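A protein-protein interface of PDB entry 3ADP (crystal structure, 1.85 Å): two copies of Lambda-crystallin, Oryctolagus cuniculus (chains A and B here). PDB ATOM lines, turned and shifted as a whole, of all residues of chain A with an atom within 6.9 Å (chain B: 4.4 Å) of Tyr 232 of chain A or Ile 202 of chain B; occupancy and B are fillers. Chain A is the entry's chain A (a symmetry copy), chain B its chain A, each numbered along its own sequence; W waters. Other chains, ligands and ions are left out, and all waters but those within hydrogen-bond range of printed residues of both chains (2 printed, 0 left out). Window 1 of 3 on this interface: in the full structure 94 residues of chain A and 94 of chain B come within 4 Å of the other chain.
The guanidinium group (NH1) of Arg 231 of chain A is in hydrogen-bond range of the side-chain amide oxygen (OE1) of Gln 199 of chain B, at 3.2 Å.
The side-chain amino group of Lys 313 of chain A lies within hydrogen-bond range of the backbone carbonyl oxygen of Ser 225 of chain B (2.8 Å).
O of Tyr 232 of chain A lies close to O of Met 224 of chain B (3.5 Å).
The backbone carbonyl oxygen (O) of Ala 233 of chain A lies close to the backbone carbonyl oxygen (O) of Ser 225 of chain B, at 3.2 Å.
The backbone carbonyl oxygen (O) of Met 224 of chain B lies within hydrogen-bond range of the backbone NH (N) of Gly 229 of chain B (2.6 Å).
N of Gly 229 of chain A lies within hydrogen-bond range of O of Met 224 of chain A (2.6 Å).
The side-chain amino group of Lys 313 of chain A is in hydrogen-bond range of the backbone carbonyl oxygen of Ala 233 of chain A.
OG1 of Thr 240 of chain A lies within hydrogen-bond range of O of Gly 236 of chain A (2.6 Å).
Water W2 lies within hydrogen-bond range of the side-chain hydroxyl of Tyr 232 of chain A (2.7 Å), the side-chain amide oxygen of Gln 199 of chain B (2.8 Å) and the backbone carbonyl oxygen of Pro 237 of chain A (2.9 Å).
Water W1 bridges NH1 of Arg 231 of chain A (3.1 Å) and NE2 of Gln 199 of chain B (3.3 Å).
Ala 201 of chain A touches its own counterpart, Ala 201 of chain B.
Ile 202 of chain A touches its own counterpart, Ile 202 of chain B.
Gly 229 of chain B touches its own counterpart, Gly 229 of chain A.
Positions printed for both chains: 198, 199, 201, 202, 224 and 229.
Of the 21 pairs that touch across the chains among the printed residues, 3 have their exchanged pair printed and touching as well.
Met 230 of chain A touches none of the printed residues of chain B.
Of chain B, only Gln 199 (3.5 Å), Ile 202 (3.4 Å), Met 224 (3.5 Å), Ser 225 (3.2 Å) and Gly 229 (3.4 Å) come within 4 Å of Tyr 232 of chain A.
Of the printed residues of chain B, Ala 233 of chain A touches Ser 225 and Gly 229.
Leu 238 of chain A touches none of the printed residues of chain B.
Of the printed residues of chain A, Tyr 200 of chain B touches Leu 263.
Of chain A, only Ile 202 (3.1 Å), Tyr 232 (3.4 Å) and Pro 237 (3.9 Å) come within 4 Å of Ile 202 of chain B.
The nearest residue of chain A that does not touch Ile 202 of chain B is Leu 198 of chain A (4.2 Å).
The nearest printed residue of chain A that does not touch Tyr 200 of chain B is Phe 266 of chain A (5.1 Å).
Of the 21 printed residues of chain A, 14 touch a printed residue of chain B.
Printed residues of chain A that touch a printed residue of chain B: Ala 201, Ile 202, Leu 228, Gly 229, Arg 231, Tyr 232, Ala 233, Phe 234, Ile 235, Pro 237, Thr 240, Leu 263, Phe 266 and Lys 313.
Of the 12 printed residues of chain B, 8 touch a printed residue of chain A.
Hydrophobic or aromatic side chains of chain B within 4 Å of the printed part of chain A: Ala 201, Ile 202 and Met 224.
Among the printed residues, no Asp or Glu carboxylate lies within 4 Å of a Lys or Arg side-chain nitrogen of the other chain.
Among the printed residues, pairs that only touch across the chains: Ile 202 of chain A with Ile 202 of chain B (3.1 Å), Tyr 232 of chain A with Ser 225 of chain B (3.2 Å), Tyr 232 of chain A with Gly 229 of chain B (3.4 Å), Tyr 232 of chain A with Ile 202 of chain B (3.4 Å), Tyr 232 of chain A with Gln 199 of chain B (3.5 Å), Phe 234 of chain A with Ser 225 of chain B (3.5 Å), Leu 263 of chain A with Tyr 200 of chain B (3.6 Å), Gly 229 of chain A with Gly 229 of chain B (3.7 Å), Thr 240 of chain A with Gln 199 of chain B (3.7 Å), Leu 263 of chain A with Ser 204 of chain B (3.7 Å), Phe 266 of chain A with Ala 201 of chain B (3.7 Å), Pro 237 of chain A with Met 224 of chain B (3.8 Å), Ile 235 of chain A with Ser 225 of chain B (3.8 Å), Ala 233 of chain A with Gly 229 of chain B (3.8 Å), Leu 228 of chain A with Gln 199 of chain B (3.8 Å), Pro 237 of chain A with Ile 202 of chain B (3.9 Å) and Ala 201 of chain A with Ala 201 of chain B (3.98 Å).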
ATOM      1  N   LEU A 198     -32.225 -14.362  25.782  1.00  0.00           N
ATOM      2  CA  LEU A 198     -31.396 -15.425  25.227  1.00  0.00           C
ATOM      3  C   LEU A 198     -32.297 -16.588  24.821  1.00  0.00           C
ATOM      4  O   LEU A 198     -32.154 -17.144  23.734  1.00  0.00           O
ATOM      5  CB  LEU A 198     -30.358 -15.905  26.249  1.00  0.00           C
ATOM      6  CG  LEU A 198     -29.255 -14.925  26.663  1.00  0.00           C
ATOM      7  CD1 LEU A 198     -28.306 -15.616  27.642  1.00  0.00           C
ATOM      8  CD2 LEU A 198     -28.493 -14.446  25.437  1.00  0.00           C
ATOM      9  N   GLN A 199     -33.239 -16.945  25.688  1.00  0.00           N
ATOM     10  CA  GLN A 199     -34.144 -18.047  25.375  1.00  0.00           C
ATOM     11  C   GLN A 199     -34.924 -17.793  24.088  1.00  0.00           C
ATOM     12  O   GLN A 199     -35.019 -18.671  23.231  1.00  0.00           O
ATOM     13  CB  GLN A 199     -35.135 -18.296  26.518  1.00  0.00           C
ATOM     14  CG  GLN A 199     -35.964 -19.557  26.283  1.00  0.00           C
ATOM     15  CD  GLN A 199     -36.909 -19.902  27.413  1.00  0.00           C
ATOM     16  OE1 GLN A 199     -37.385 -21.033  27.498  1.00  0.00           O
ATOM     17  NE2 GLN A 199     -37.201 -18.931  28.276  1.00  0.00           N
ATOM     18  N   ALA A 201     -34.136 -15.876  21.666  1.00  0.00           N
ATOM     19  CA  ALA A 201     -33.217 -15.842  20.534  1.00  0.00           C
ATOM     20  C   ALA A 201     -33.106 -17.253  19.971  1.00  0.00           C
ATOM     21  O   ALA A 201     -33.161 -17.454  18.758  1.00  0.00           O
ATOM     22  CB  ALA A 201     -31.841 -15.346  20.978  1.00  0.00           C
ATOM     23  N   ILE A 202     -32.951 -18.225  20.865  1.00  0.00           N
ATOM     24  CA  ILE A 202     -32.834 -19.627  20.478  1.00  0.00           C
ATOM     25  C   ILE A 202     -34.134 -20.127  19.858  1.00  0.00           C
ATOM     26  O   ILE A 202     -34.128 -20.721  18.783  1.00  0.00           O
ATOM     27  CB  ILE A 202     -32.499 -20.516  21.697  1.00  0.00           C
ATOM     28  CG1 ILE A 202     -31.146 -20.105  22.278  1.00  0.00           C
ATOM     29  CG2 ILE A 202     -32.479 -21.987  21.285  1.00  0.00           C
ATOM     30  CD1 ILE A 202     -30.872 -20.666  23.662  1.00  0.00           C
ATOM     31  N   MET A 224     -29.792 -29.816  21.187  1.00  0.00           N
ATOM     32  CA  MET A 224     -29.520 -29.046  22.389  1.00  0.00           C
ATOM     33  C   MET A 224     -29.240 -29.943  23.597  1.00  0.00           C
ATOM     34  O   MET A 224     -28.153 -29.886  24.170  1.00  0.00           O
ATOM     35  CB  MET A 224     -30.702 -28.118  22.702  1.00  0.00           C
ATOM     36  CG  MET A 224     -30.506 -27.223  23.929  1.00  0.00           C
ATOM     37  SD  MET A 224     -29.176 -25.997  23.766  1.00  0.00           S
ATOM     38  CE  MET A 224     -30.063 -24.634  22.980  1.00  0.00           C
ATOM     39  N   GLY A 227     -26.329 -32.143  23.028  1.00  0.00           N
ATOM     40  CA  GLY A 227     -25.237 -31.469  22.323  1.00  0.00           C
ATOM     41  C   GLY A 227     -24.836 -30.138  22.979  1.00  0.00           C
ATOM     42  O   GLY A 227     -24.161 -30.102  24.000  1.00  0.00           O
ATOM     43  N   LEU A 228     -25.259 -29.045  22.354  1.00  0.00           N
ATOM     44  CA  LEU A 228     -24.919 -27.706  22.815  1.00  0.00           C
ATOM     45  C   LEU A 228     -25.300 -27.428  24.267  1.00  0.00           C
ATOM     46  O   LEU A 228     -24.559 -26.758  24.992  1.00  0.00           O
ATOM     47  CB  LEU A 228     -25.580 -26.673  21.898  1.00  0.00           C
ATOM     48  CG  LEU A 228     -25.233 -25.202  22.138  1.00  0.00           C
ATOM     49  CD1 LEU A 228     -23.743 -24.981  21.923  1.00  0.00           C
ATOM     50  CD2 LEU A 228     -26.050 -24.335  21.187  1.00  0.00           C
ATOM     51  N   GLY A 229     -26.450 -27.943  24.685  1.00  0.00           N
ATOM     52  CA  GLY A 229     -26.915 -27.720  26.045  1.00  0.00           C
ATOM     53  C   GLY A 229     -26.012 -28.283  27.125  1.00  0.00           C
ATOM     54  O   GLY A 229     -25.942 -27.746  28.229  1.00  0.00           O
ATOM     55  N   MET A 230     -25.314 -29.368  26.816  1.00  0.00           N
ATOM     56  CA  MET A 230     -24.429 -29.980  27.797  1.00  0.00           C
ATOM     57  C   MET A 230     -23.306 -29.037  28.209  1.00  0.00           C
ATOM     58  O   MET A 230     -22.961 -28.951  29.387  1.00  0.00           O
ATOM     59  CB  MET A 230     -23.856 -31.284  27.244  1.00  0.00           C
ATOM     60  CG  MET A 230     -24.898 -32.382  27.113  1.00  0.00           C
ATOM     61  SD  MET A 230     -24.224 -33.949  26.527  1.00  0.00           S
ATOM     62  CE  MET A 230     -23.233 -34.448  27.943  1.00  0.00           C
ATOM     63  N   ARG A 231     -22.742 -28.317  27.246  1.00  0.00           N
ATOM     64  CA  ARG A 231     -21.665 -27.386  27.561  1.00  0.00           C
ATOM     65  C   ARG A 231     -22.228 -26.196  28.335  1.00  0.00           C
ATOM     66  O   ARG A 231     -21.601 -25.698  29.268  1.00  0.00           O
ATOM     67  CB  ARG A 231     -20.980 -26.891  26.282  1.00  0.00           C
ATOM     68  CG  ARG A 231     -21.749 -25.819  25.525  1.00  0.00           C
ATOM     69  CD  ARG A 231     -21.030 -25.394  24.250  1.00  0.00           C
ATOM     70  NE  ARG A 231     -21.019 -26.454  23.245  1.00  0.00           N
ATOM     71  CZ  ARG A 231     -20.547 -26.316  22.007  1.00  0.00           C
ATOM     72  NH1 ARG A 231     -20.040 -25.156  21.605  1.00  0.00           N
ATOM     73  NH2 ARG A 231     -20.595 -27.338  21.164  1.00  0.00           N
ATOM     74  N   TYR A 232     -23.427 -25.761  27.956  1.00  0.00           N
ATOM     75  CA  TYR A 232     -24.038 -24.575  28.548  1.00  0.00           C
ATOM     76  C   TYR A 232     -24.449 -24.789  30.011  1.00  0.00           C
ATOM     77  O   TYR A 232     -24.820 -23.863  30.719  1.00  0.00           O
ATOM     78  CB  TYR A 232     -25.267 -24.200  27.722  1.00  0.00           C
ATOM     79  CG  TYR A 232     -24.884 -23.469  26.480  1.00  0.00           C
ATOM     80  CD1 TYR A 232     -23.590 -22.980  26.309  1.00  0.00           C
ATOM     81  CD2 TYR A 232     -25.841 -23.252  25.490  1.00  0.00           C
ATOM     82  CE1 TYR A 232     -23.258 -22.292  25.147  1.00  0.00           C
ATOM     83  CE2 TYR A 232     -25.512 -22.557  24.336  1.00  0.00           C
ATOM     84  CZ  TYR A 232     -24.227 -22.075  24.164  1.00  0.00           C
ATOM     85  OH  TYR A 232     -23.888 -21.394  23.010  1.00  0.00           O
ATOM     86  N   ALA A 233     -24.433 -26.067  30.448  1.00  0.00           N
ATOM     87  CA  ALA A 233     -24.773 -26.332  31.848  1.00  0.00           C
ATOM     88  C   ALA A 233     -23.604 -26.016  32.788  1.00  0.00           C
ATOM     89  O   ALA A 233     -23.736 -25.996  34.002  1.00  0.00           O
ATOM     90  CB  ALA A 233     -25.170 -27.806  31.976  1.00  0.00           C
ATOM     91  N   PHE A 234     -22.418 -25.791  32.183  1.00  0.00           N
ATOM     92  CA  PHE A 234     -21.217 -25.518  32.964  1.00  0.00           C
ATOM     93  C   PHE A 234     -20.573 -24.190  32.549  1.00  0.00           C
ATOM     94  O   PHE A 234     -19.957 -23.488  33.340  1.00  0.00           O
ATOM     95  CB  PHE A 234     -20.228 -26.673  32.758  1.00  0.00           C
ATOM     96  CG  PHE A 234     -20.803 -27.958  33.286  1.00  0.00           C
ATOM     97  CD1 PHE A 234     -20.924 -28.146  34.658  1.00  0.00           C
ATOM     98  CD2 PHE A 234     -21.198 -28.952  32.406  1.00  0.00           C
ATOM     99  CE1 PHE A 234     -21.443 -29.335  35.147  1.00  0.00           C
ATOM    100  CE2 PHE A 234     -21.720 -30.142  32.905  1.00  0.00           C
ATOM    101  CZ  PHE A 234     -21.844 -30.340  34.275  1.00  0.00           C
ATOM    102  N   ILE A 235     -20.632 -23.842  31.270  1.00  0.00           N
ATOM    103  CA  ILE A 235     -19.970 -22.638  30.782  1.00  0.00           C
ATOM    104  C   ILE A 235     -20.874 -21.856  29.834  1.00  0.00           C
ATOM    105  O   ILE A 235     -21.528 -22.439  28.971  1.00  0.00           O
ATOM    106  CB  ILE A 235     -18.653 -23.010  30.064  1.00  0.00           C
ATOM    107  CG1 ILE A 235     -17.687 -23.650  31.067  1.00  0.00           C
ATOM    108  CG2 ILE A 235     -18.020 -21.777  29.436  1.00  0.00           C
ATOM    109  CD1 ILE A 235     -16.418 -24.184  30.450  1.00  0.00           C
ATOM    110  N   GLY A 236     -20.900 -20.537  30.006  1.00  0.00           N
ATOM    111  CA  GLY A 236     -21.728 -19.678  29.175  1.00  0.00           C
ATOM    112  C   GLY A 236     -21.310 -19.621  27.715  1.00  0.00           C
ATOM    113  O   GLY A 236     -20.262 -20.142  27.345  1.00  0.00           O
ATOM    114  N   PRO A 237     -22.108 -18.967  26.858  1.00  0.00           N
ATOM    115  CA  PRO A 237     -21.788 -18.866  25.430  1.00  0.00           C
ATOM    116  C   PRO A 237     -20.501 -18.112  25.097  1.00  0.00           C
ATOM    117  O   PRO A 237     -19.838 -18.424  24.107  1.00  0.00           O
ATOM    118  CB  PRO A 237     -23.024 -18.188  24.851  1.00  0.00           C
ATOM    119  CG  PRO A 237     -23.450 -17.281  25.975  1.00  0.00           C
ATOM    120  CD  PRO A 237     -23.319 -18.190  27.182  1.00  0.00           C
ATOM    121  N   LEU A 238     -20.142 -17.126  25.915  1.00  0.00           N
ATOM    122  CA  LEU A 238     -18.933 -16.356  25.655  1.00  0.00           C
ATOM    123  C   LEU A 238     -17.682 -17.130  26.049  1.00  0.00           C
ATOM    124  O   LEU A 238     -16.740 -17.232  25.263  1.00  0.00           O
ATOM    125  CB  LEU A 238     -18.994 -15.010  26.387  1.00  0.00           C
ATOM    126  CG  LEU A 238     -20.181 -14.127  25.984  1.00  0.00           C
ATOM    127  CD1 LEU A 238     -20.133 -12.820  26.760  1.00  0.00           C
ATOM    128  CD2 LEU A 238     -20.151 -13.860  24.481  1.00  0.00           C
ATOM    129  N   THR A 240     -17.474 -20.175  26.258  1.00  0.00           N
ATOM    130  CA  THR A 240     -17.457 -21.330  25.362  1.00  0.00           C
ATOM    131  C   THR A 240     -16.639 -20.996  24.112  1.00  0.00           C
ATOM    132  O   THR A 240     -15.845 -21.815  23.641  1.00  0.00           O
ATOM    133  CB  THR A 240     -18.888 -21.738  24.953  1.00  0.00           C
ATOM    134  OG1 THR A 240     -19.549 -22.335  26.077  1.00  0.00           O
ATOM    135  CG2 THR A 240     -18.865 -22.727  23.798  1.00  0.00           C
ATOM    136  N   LEU A 263     -25.724 -15.768  10.349  1.00  0.00           N
ATOM    137  CA  LEU A 263     -26.704 -14.842  10.909  1.00  0.00           C
ATOM    138  C   LEU A 263     -27.425 -14.033   9.832  1.00  0.00           C
ATOM    139  O   LEU A 263     -28.619 -13.751   9.944  1.00  0.00           O
ATOM    140  CB  LEU A 263     -26.024 -13.910  11.921  1.00  0.00           C
ATOM    141  CG  LEU A 263     -25.534 -14.595  13.209  1.00  0.00           C
ATOM    142  CD1 LEU A 263     -24.667 -13.640  14.022  1.00  0.00           C
ATOM    143  CD2 LEU A 263     -26.733 -15.058  14.030  1.00  0.00           C
ATOM    144  N   PHE A 266     -30.548 -15.669   8.470  1.00  0.00           N
ATOM    145  CA  PHE A 266     -31.706 -15.859   9.344  1.00  0.00           C
ATOM    146  C   PHE A 266     -32.974 -15.239   8.764  1.00  0.00           C
ATOM    147  O   PHE A 266     -32.953 -14.114   8.261  1.00  0.00           O
ATOM    148  CB  PHE A 266     -31.434 -15.249  10.722  1.00  0.00           C
ATOM    149  CG  PHE A 266     -30.712 -16.171  11.669  1.00  0.00           C
ATOM    150  CD1 PHE A 266     -29.872 -17.174  11.193  1.00  0.00           C
ATOM    151  CD2 PHE A 266     -30.858 -16.018  13.044  1.00  0.00           C
ATOM    152  CE1 PHE A 266     -29.186 -18.012  12.074  1.00  0.00           C
ATOM    153  CE2 PHE A 266     -30.176 -16.852  13.936  1.00  0.00           C
ATOM    154  CZ  PHE A 266     -29.339 -17.851  13.448  1.00  0.00           C
ATOM    155  N   LYS A 313     -22.706 -29.662  39.850  1.00  0.00           N
ATOM    156  CA  LYS A 313     -22.053 -28.367  39.676  1.00  0.00           C
ATOM    157  C   LYS A 313     -21.350 -27.915  40.957  1.00  0.00           C
ATOM    158  O   LYS A 313     -20.219 -27.425  40.915  1.00  0.00           O
ATOM    159  CB  LYS A 313     -23.076 -27.318  39.220  1.00  0.00           C
ATOM    160  CG  LYS A 313     -23.554 -27.530  37.782  1.00  0.00           C
ATOM    161  CD  LYS A 313     -24.820 -26.735  37.460  1.00  0.00           C
ATOM    162  CE  LYS A 313     -24.601 -25.232  37.552  1.00  0.00           C
ATOM    163  NZ  LYS A 313     -23.618 -24.740  36.550  1.00  0.00           N
ATOM    164  N   LEU B 198     -27.904 -22.547  16.055  1.00  0.00           N
ATOM    165  CA  LEU B 198     -28.475 -22.240  17.360  1.00  0.00           C
ATOM    166  C   LEU B 198     -27.428 -21.508  18.193  1.00  0.00           C
ATOM    167  O   LEU B 198     -27.725 -20.500  18.833  1.00  0.00           O
ATOM    168  CB  LEU B 198     -28.913 -23.519  18.085  1.00  0.00           C
ATOM    169  CG  LEU B 198     -30.079 -24.315  17.489  1.00  0.00           C
ATOM    170  CD1 LEU B 198     -30.383 -25.515  18.386  1.00  0.00           C
ATOM    171  CD2 LEU B 198     -31.307 -23.428  17.359  1.00  0.00           C
ATOM    172  N   GLN B 199     -26.195 -22.003  18.174  1.00  0.00           N
ATOM    173  CA  GLN B 199     -25.134 -21.360  18.943  1.00  0.00           C
ATOM    174  C   GLN B 199     -24.937 -19.904  18.531  1.00  0.00           C
ATOM    175  O   GLN B 199     -24.844 -19.021  19.383  1.00  0.00           O
ATOM    176  CB  GLN B 199     -23.803 -22.106  18.787  1.00  0.00           C
ATOM    177  CG  GLN B 199     -22.732 -21.554  19.726  1.00  0.00           C
ATOM    178  CD  GLN B 199     -21.416 -22.297  19.677  1.00  0.00           C
ATOM    179  OE1 GLN B 199     -20.598 -22.169  20.587  1.00  0.00           O
ATOM    180  NE2 GLN B 199     -21.193 -23.065  18.612  1.00  0.00           N
ATOM    181  N   TYR B 200     -24.868 -19.648  17.227  1.00  0.00           N
ATOM    182  CA  TYR B 200     -24.664 -18.282  16.748  1.00  0.00           C
ATOM    183  C   TYR B 200     -25.846 -17.385  17.084  1.00  0.00           C
ATOM    184  O   TYR B 200     -25.677 -16.185  17.303  1.00  0.00           O
ATOM    185  CB  TYR B 200     -24.418 -18.265  15.238  1.00  0.00           C
ATOM    186  CG  TYR B 200     -23.162 -18.984  14.788  1.00  0.00           C
ATOM    187  CD1 TYR B 200     -22.191 -19.398  15.706  1.00  0.00           C
ATOM    188  CD2 TYR B 200     -22.938 -19.236  13.437  1.00  0.00           C
ATOM    189  CE1 TYR B 200     -21.026 -20.050  15.281  1.00  0.00           C
ATOM    190  CE2 TYR B 200     -21.785 -19.880  13.002  1.00  0.00           C
ATOM    191  CZ  TYR B 200     -20.833 -20.284  13.924  1.00  0.00           C
ATOM    192  OH  TYR B 200     -19.697 -20.915  13.479  1.00  0.00           O
ATOM    193  N   ALA B 201     -27.041 -17.965  17.124  1.00  0.00           N
ATOM    194  CA  ALA B 201     -28.234 -17.196  17.458  1.00  0.00           C
ATOM    195  C   ALA B 201     -28.055 -16.631  18.863  1.00  0.00           C
ATOM    196  O   ALA B 201     -28.333 -15.458  19.110  1.00  0.00           O
ATOM    197  CB  ALA B 201     -29.475 -18.086  17.406  1.00  0.00           C
ATOM    198  N   ILE B 202     -27.590 -17.479  19.775  1.00  0.00           N
ATOM    199  CA  ILE B 202     -27.363 -17.082  21.161  1.00  0.00           C
ATOM    200  C   ILE B 202     -26.245 -16.051  21.253  1.00  0.00           C
ATOM    201  O   ILE B 202     -26.404 -15.008  21.883  1.00  0.00           O
ATOM    202  CB  ILE B 202     -26.980 -18.300  22.033  1.00  0.00           C
ATOM    203  CG1 ILE B 202     -28.130 -19.308  22.045  1.00  0.00           C
ATOM    204  CG2 ILE B 202     -26.653 -17.845  23.455  1.00  0.00           C
ATOM    205  CD1 ILE B 202     -27.745 -20.676  22.577  1.00  0.00           C
ATOM    206  N   ILE B 203     -25.112 -16.350  20.625  1.00  0.00           N
ATOM    207  CA  ILE B 203     -23.961 -15.445  20.643  1.00  0.00           C
ATOM    208  C   ILE B 203     -24.302 -14.041  20.133  1.00  0.00           C
ATOM    209  O   ILE B 203     -23.856 -13.042  20.701  1.00  0.00           O
ATOM    210  CB  ILE B 203     -22.796 -16.026  19.805  1.00  0.00           C
ATOM    211  CG1 ILE B 203     -22.265 -17.296  20.482  1.00  0.00           C
ATOM    212  CG2 ILE B 203     -21.673 -14.989  19.658  1.00  0.00           C
ATOM    213  CD1 ILE B 203     -21.163 -18.003  19.714  1.00  0.00           C
ATOM    214  N   SER B 204     -25.098 -13.965  19.071  1.00  0.00           N
ATOM    215  CA  SER B 204     -25.484 -12.683  18.492  1.00  0.00           C
ATOM    216  C   SER B 204     -26.204 -11.784  19.501  1.00  0.00           C
ATOM    217  O   SER B 204     -25.852 -10.617  19.663  1.00  0.00           O
ATOM    218  CB  SER B 204     -26.378 -12.911  17.269  1.00  0.00           C
ATOM    219  OG  SER B 204     -26.614 -11.696  16.576  1.00  0.00           O
ATOM    220  N   GLU B 205     -27.208 -12.329  20.181  1.00  0.00           N
ATOM    221  CA  GLU B 205     -27.960 -11.555  21.169  1.00  0.00           C
ATOM    222  C   GLU B 205     -27.092 -11.263  22.392  1.00  0.00           C
ATOM    223  O   GLU B 205     -27.116 -10.153  22.923  1.00  0.00           O
ATOM    224  CB  GLU B 205     -29.234 -12.312  21.570  1.00  0.00           C
ATOM    225  CG  GLU B 205     -30.027 -11.713  22.739  1.00  0.00           C
ATOM    226  CD  GLU B 205     -30.428 -10.261  22.529  1.00  0.00           C
ATOM    227  OE1 GLU B 205     -30.392  -9.782  21.376  1.00  0.00           O
ATOM    228  OE2 GLU B 205     -30.795  -9.601  23.527  1.00  0.00           O
ATOM    229  N   ALA B 206     -26.317 -12.251  22.834  1.00  0.00           N
ATOM    230  CA  ALA B 206     -25.444 -12.056  23.987  1.00  0.00           C
ATOM    231  C   ALA B 206     -24.472 -10.906  23.726  1.00  0.00           C
ATOM    232  O   ALA B 206     -24.240 -10.060  24.595  1.00  0.00           O
ATOM    233  CB  ALA B 206     -24.665 -13.337  24.281  1.00  0.00           C
ATOM    234  N   MET B 224     -26.533 -18.244  31.722  1.00  0.00           N
ATOM    235  CA  MET B 224     -26.637 -19.505  31.007  1.00  0.00           C
ATOM    236  C   MET B 224     -26.206 -20.694  31.870  1.00  0.00           C
ATOM    237  O   MET B 224     -27.007 -21.590  32.132  1.00  0.00           O
ATOM    238  CB  MET B 224     -25.787 -19.462  29.730  1.00  0.00           C
ATOM    239  CG  MET B 224     -25.856 -20.728  28.872  1.00  0.00           C
ATOM    240  SD  MET B 224     -27.490 -21.066  28.153  1.00  0.00           S
ATOM    241  CE  MET B 224     -27.396 -20.101  26.629  1.00  0.00           C
ATOM    242  N   SER B 225     -24.956 -20.684  32.334  1.00  0.00           N
ATOM    243  CA  SER B 225     -24.411 -21.806  33.115  1.00  0.00           C
ATOM    244  C   SER B 225     -25.150 -22.108  34.426  1.00  0.00           C
ATOM    245  O   SER B 225     -25.254 -23.253  34.847  1.00  0.00           O
ATOM    246  CB  SER B 225     -22.908 -21.618  33.350  1.00  0.00           C
ATOM    247  OG  SER B 225     -22.666 -20.530  34.253  1.00  0.00           O
ATOM    248  N   GLY B 229     -28.986 -22.724  30.813  1.00  0.00           N
ATOM    249  CA  GLY B 229     -28.207 -23.868  30.368  1.00  0.00           C
ATOM    250  C   GLY B 229     -28.479 -25.154  31.123  1.00  0.00           C
ATOM    251  O   GLY B 229     -28.359 -26.246  30.571  1.00  0.00           O
HETATM  252  O   HOH W   1     -19.012 -25.513  18.693  1.00  0.00           O
HETATM  253  O   HOH W   2     -21.380 -20.371  22.618  1.00  0.00           O
